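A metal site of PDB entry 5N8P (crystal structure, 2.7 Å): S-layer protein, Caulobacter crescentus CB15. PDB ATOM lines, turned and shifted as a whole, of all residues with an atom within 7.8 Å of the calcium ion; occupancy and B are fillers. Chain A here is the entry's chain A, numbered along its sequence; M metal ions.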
ATOM      1  N   SER A 253     -18.450 -10.988  12.092  1.00  0.00           N
ATOM      2  CA  SER A 253     -18.563  -9.770  11.310  1.00  0.00           C
ATOM      3  C   SER A 253     -19.446  -8.675  11.913  1.00  0.00           C
ATOM      4  O   SER A 253     -20.625  -8.903  12.116  1.00  0.00           O
ATOM      5  CB  SER A 253     -19.132 -10.112   9.949  1.00  0.00           C
ATOM      6  OG  SER A 253     -18.087 -10.457   9.096  1.00  0.00           O
ATOM      7  N   LEU A 254     -18.872  -7.480  12.090  1.00  0.00           N
ATOM      8  CA  LEU A 254     -19.641  -6.303  12.496  1.00  0.00           C
ATOM      9  C   LEU A 254     -20.480  -5.781  11.344  1.00  0.00           C
ATOM     10  O   LEU A 254     -20.101  -5.956  10.201  1.00  0.00           O
ATOM     11  CB  LEU A 254     -18.724  -5.189  12.999  1.00  0.00           C
ATOM     12  CG  LEU A 254     -18.312  -5.194  14.486  1.00  0.00           C
ATOM     13  CD1 LEU A 254     -17.288  -6.260  14.767  1.00  0.00           C
ATOM     14  CD2 LEU A 254     -17.740  -3.844  14.878  1.00  0.00           C
ATOM     15  N   THR A 255     -21.629  -5.158  11.639  1.00  0.00           N
ATOM     16  CA  THR A 255     -22.535  -4.555  10.641  1.00  0.00           C
ATOM     17  C   THR A 255     -22.640  -3.054  10.799  1.00  0.00           C
ATOM     18  O   THR A 255     -22.113  -2.515  11.764  1.00  0.00           O
ATOM     19  CB  THR A 255     -23.959  -5.092  10.753  1.00  0.00           C
ATOM     20  OG1 THR A 255     -24.600  -4.440  11.859  1.00  0.00           O
ATOM     21  CG2 THR A 255     -23.945  -6.621  10.951  1.00  0.00           C
ATOM     22  N   THR A 256     -23.344  -2.367   9.914  1.00  0.00           N
ATOM     23  CA  THR A 256     -23.489  -0.911  10.088  1.00  0.00           C
ATOM     24  C   THR A 256     -24.423  -0.578  11.276  1.00  0.00           C
ATOM     25  O   THR A 256     -24.674   0.610  11.536  1.00  0.00           O
ATOM     26  CB  THR A 256     -24.018  -0.189   8.831  1.00  0.00           C
ATOM     27  OG1 THR A 256     -25.311  -0.675   8.525  1.00  0.00           O
ATOM     28  CG2 THR A 256     -23.158  -0.487   7.634  1.00  0.00           C
ATOM     29  N   GLY A 257     -24.890  -1.590  12.002  1.00  0.00           N
ATOM     30  CA  GLY A 257     -25.727  -1.393  13.198  1.00  0.00           C
ATOM     31  C   GLY A 257     -25.053  -1.354  14.589  1.00  0.00           C
ATOM     32  O   GLY A 257     -23.909  -0.947  14.726  1.00  0.00           O
ATOM     33  N   THR A 258     -25.789  -1.770  15.616  1.00  0.00           N
ATOM     34  CA  THR A 258     -25.217  -1.990  16.911  1.00  0.00           C
ATOM     35  C   THR A 258     -25.043  -3.472  17.151  1.00  0.00           C
ATOM     36  O   THR A 258     -26.004  -4.222  17.223  1.00  0.00           O
ATOM     37  CB  THR A 258     -26.073  -1.329  18.016  1.00  0.00           C
ATOM     38  OG1 THR A 258     -26.024   0.075  17.820  1.00  0.00           O
ATOM     39  CG2 THR A 258     -25.522  -1.656  19.388  1.00  0.00           C
ATOM     40  N   ASP A 259     -23.773  -3.884  17.284  1.00  0.00           N
ATOM     41  CA  ASP A 259     -23.459  -5.297  17.382  1.00  0.00           C
ATOM     42  C   ASP A 259     -23.142  -5.682  18.797  1.00  0.00           C
ATOM     43  O   ASP A 259     -22.489  -4.947  19.533  1.00  0.00           O
ATOM     44  CB  ASP A 259     -22.303  -5.609  16.452  1.00  0.00           C
ATOM     45  CG  ASP A 259     -22.566  -5.127  15.020  1.00  0.00           C
ATOM     46  OD1 ASP A 259     -23.403  -5.752  14.299  1.00  0.00           O
ATOM     47  OD2 ASP A 259     -21.999  -4.092  14.631  1.00  0.00           O
ATOM     48  N   THR A 260     -23.601  -6.870  19.185  1.00  0.00           N
ATOM     49  CA  THR A 260     -23.278  -7.448  20.477  1.00  0.00           C
ATOM     50  C   THR A 260     -22.664  -8.833  20.241  1.00  0.00           C
ATOM     51  O   THR A 260     -23.354  -9.853  20.172  1.00  0.00           O
ATOM     52  CB  THR A 260     -24.489  -7.447  21.433  1.00  0.00           C
ATOM     53  OG1 THR A 260     -25.078  -6.130  21.431  1.00  0.00           O
ATOM     54  CG2 THR A 260     -24.065  -7.802  22.866  1.00  0.00           C
ATOM     55  N   LEU A 261     -21.340  -8.866  20.120  1.00  0.00           N
ATOM     56  CA  LEU A 261     -20.634 -10.048  19.664  1.00  0.00           C
ATOM     57  C   LEU A 261     -19.780 -10.636  20.764  1.00  0.00           C
ATOM     58  O   LEU A 261     -19.088  -9.912  21.482  1.00  0.00           O
ATOM     59  CB  LEU A 261     -19.811  -9.729  18.424  1.00  0.00           C
ATOM     60  CG  LEU A 261     -20.545  -9.179  17.206  1.00  0.00           C
ATOM     61  CD1 LEU A 261     -19.610  -8.883  16.041  1.00  0.00           C
ATOM     62  CD2 LEU A 261     -21.728 -10.070  16.760  1.00  0.00           C
ATOM     63  N   ALA A 272     -14.181  -5.710  11.442  1.00  0.00           N
ATOM     64  CA  ALA A 272     -14.869  -4.444  11.453  1.00  0.00           C
ATOM     65  C   ALA A 272     -14.571  -3.649  10.194  1.00  0.00           C
ATOM     66  O   ALA A 272     -14.091  -2.521  10.242  1.00  0.00           O
ATOM     67  CB  ALA A 272     -14.521  -3.670  12.682  1.00  0.00           C
ATOM     68  N   ALA A 279     -18.740   2.354   7.327  1.00  0.00           N
ATOM     69  CA  ALA A 279     -18.020   1.799   8.480  1.00  0.00           C
ATOM     70  C   ALA A 279     -18.849   0.800   9.287  1.00  0.00           C
ATOM     71  O   ALA A 279     -20.073   1.003   9.393  1.00  0.00           O
ATOM     72  CB  ALA A 279     -17.578   2.926   9.375  1.00  0.00           C
ATOM     73  N   THR A 280     -18.236  -0.254   9.818  1.00  0.00           N
ATOM     74  CA  THR A 280     -19.007  -1.181  10.680  1.00  0.00           C
ATOM     75  C   THR A 280     -18.702  -1.139  12.180  1.00  0.00           C
ATOM     76  O   THR A 280     -19.404  -1.772  12.981  1.00  0.00           O
ATOM     77  CB  THR A 280     -19.045  -2.644  10.190  1.00  0.00           C
ATOM     78  OG1 THR A 280     -17.764  -3.267  10.368  1.00  0.00           O
ATOM     79  CG2 THR A 280     -19.492  -2.722   8.757  1.00  0.00           C
ATOM     80  N   LEU A 281     -17.662  -0.418  12.576  1.00  0.00           N
ATOM     81  CA  LEU A 281     -17.506  -0.082  13.988  1.00  0.00           C
ATOM     82  C   LEU A 281     -18.254   1.222  14.209  1.00  0.00           C
ATOM     83  O   LEU A 281     -17.878   2.272  13.681  1.00  0.00           O
ATOM     84  CB  LEU A 281     -16.057  -0.033  14.431  1.00  0.00           C
ATOM     85  CG  LEU A 281     -15.822  -0.127  15.927  1.00  0.00           C
ATOM     86  CD1 LEU A 281     -15.750  -1.555  16.430  1.00  0.00           C
ATOM     87  CD2 LEU A 281     -14.514   0.553  16.261  1.00  0.00           C
ATOM     88  N   THR A 282     -19.349   1.122  14.948  1.00  0.00           N
ATOM     89  CA  THR A 282     -20.364   2.185  15.053  1.00  0.00           C
ATOM     90  C   THR A 282     -20.911   2.257  16.455  1.00  0.00           C
ATOM     91  O   THR A 282     -20.632   1.373  17.293  1.00  0.00           O
ATOM     92  CB  THR A 282     -21.556   1.870  14.161  1.00  0.00           C
ATOM     93  OG1 THR A 282     -21.827   0.471  14.266  1.00  0.00           O
ATOM     94  CG2 THR A 282     -21.261   2.209  12.693  1.00  0.00           C
ATOM     95  N   VAL A 283     -21.738   3.269  16.714  1.00  0.00           N
ATOM     96  CA  VAL A 283     -22.243   3.538  18.053  1.00  0.00           C
ATOM     97  C   VAL A 283     -22.824   2.316  18.774  1.00  0.00           C
ATOM     98  O   VAL A 283     -23.583   1.573  18.204  1.00  0.00           O
ATOM     99  CB  VAL A 283     -23.112   4.848  18.128  1.00  0.00           C
ATOM    100  CG1 VAL A 283     -22.922   5.768  16.912  1.00  0.00           C
ATOM    101  CG2 VAL A 283     -24.558   4.540  18.136  1.00  0.00           C
ATOM    102  N   GLY A 284     -22.379   2.098  20.018  1.00  0.00           N
ATOM    103  CA  GLY A 284     -22.905   1.059  20.902  1.00  0.00           C
ATOM    104  C   GLY A 284     -22.345  -0.336  20.709  1.00  0.00           C
ATOM    105  O   GLY A 284     -22.640  -1.222  21.543  1.00  0.00           O
ATOM    106  N   ASP A 285     -21.584  -0.550  19.639  1.00  0.00           N
ATOM    107  CA  ASP A 285     -20.944  -1.831  19.371  1.00  0.00           C
ATOM    108  C   ASP A 285     -20.234  -2.366  20.618  1.00  0.00           C
ATOM    109  O   ASP A 285     -19.357  -1.697  21.169  1.00  0.00           O
ATOM    110  CB  ASP A 285     -19.924  -1.718  18.230  1.00  0.00           C
ATOM    111  CG  ASP A 285     -20.542  -1.664  16.840  1.00  0.00           C
ATOM    112  OD1 ASP A 285     -19.808  -1.315  15.886  1.00  0.00           O
ATOM    113  OD2 ASP A 285     -21.743  -1.978  16.650  1.00  0.00           O
ATOM    114  N   THR A 286     -20.599  -3.552  21.083  1.00  0.00           N
ATOM    115  CA  THR A 286     -19.823  -4.133  22.184  1.00  0.00           C
ATOM    116  C   THR A 286     -19.307  -5.518  21.823  1.00  0.00           C
ATOM    117  O   THR A 286     -20.069  -6.408  21.421  1.00  0.00           O
ATOM    118  CB  THR A 286     -20.537  -4.072  23.578  1.00  0.00           C
ATOM    119  OG1 THR A 286     -21.573  -5.042  23.627  1.00  0.00           O
ATOM    120  CG2 THR A 286     -21.112  -2.658  23.943  1.00  0.00           C
ATOM    121  N   LEU A 287     -17.981  -5.672  21.959  1.00  0.00           N
ATOM    122  CA  LEU A 287     -17.275  -6.902  21.569  1.00  0.00           C
ATOM    123  C   LEU A 287     -16.594  -7.559  22.754  1.00  0.00           C
ATOM    124  O   LEU A 287     -16.024  -6.878  23.601  1.00  0.00           O
ATOM    125  CB  LEU A 287     -16.292  -6.637  20.418  1.00  0.00           C
ATOM    126  CG  LEU A 287     -16.731  -5.750  19.265  1.00  0.00           C
ATOM    127  CD1 LEU A 287     -15.540  -5.255  18.452  1.00  0.00           C
ATOM    128  CD2 LEU A 287     -17.792  -6.467  18.431  1.00  0.00           C
ATOM    129  N   VAL A 311     -18.999   2.314  22.361  1.00  0.00           N
ATOM    130  CA  VAL A 311     -18.167   1.190  21.940  1.00  0.00           C
ATOM    131  C   VAL A 311     -17.327   0.709  23.114  1.00  0.00           C
ATOM    132  O   VAL A 311     -16.725   1.530  23.807  1.00  0.00           O
ATOM    133  CB  VAL A 311     -17.306   1.525  20.695  1.00  0.00           C
ATOM    134  CG1 VAL A 311     -16.256   0.428  20.414  1.00  0.00           C
ATOM    135  CG2 VAL A 311     -18.179   1.692  19.468  1.00  0.00           C
HETATM  136 CA    CA M   1     -21.476  -1.911  14.110  1.00  0.00          CA
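The calcium ion is bound by the side-chain carboxylate (OD2) of Asp 259 (2.3 Å), the backbone carbonyl oxygen (O) of Thr 280 (2.4 Å), the side-chain hydroxyl (OG1) of Thr 282 (2.4 Å), the backbone carbonyl oxygen (O) of Thr 255 (2.5 Å), the side-chain carboxylate (OD1) of Asp 285 (2.5 Å), the side-chain carboxylate (OD2) of Asp 285 (2.6 Å) and the backbone carbonyl oxygen (O) of Gly 257 (2.7 Å).
Of the 20 residues printed, 6 come within 4 Å of the calcium ion. The nearest printed residue that does not touch the calcium ion is Leu 254 (4.3 Å).
OG1 of Thr 255 is in hydrogen-bond range of N of Gly 257 (2.9 Å). The backbone carbonyl oxygen (O) of Asp 259 sits at hydrogen-bond distance from the backbone NH (N) of Thr 286 (2.8 Å).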
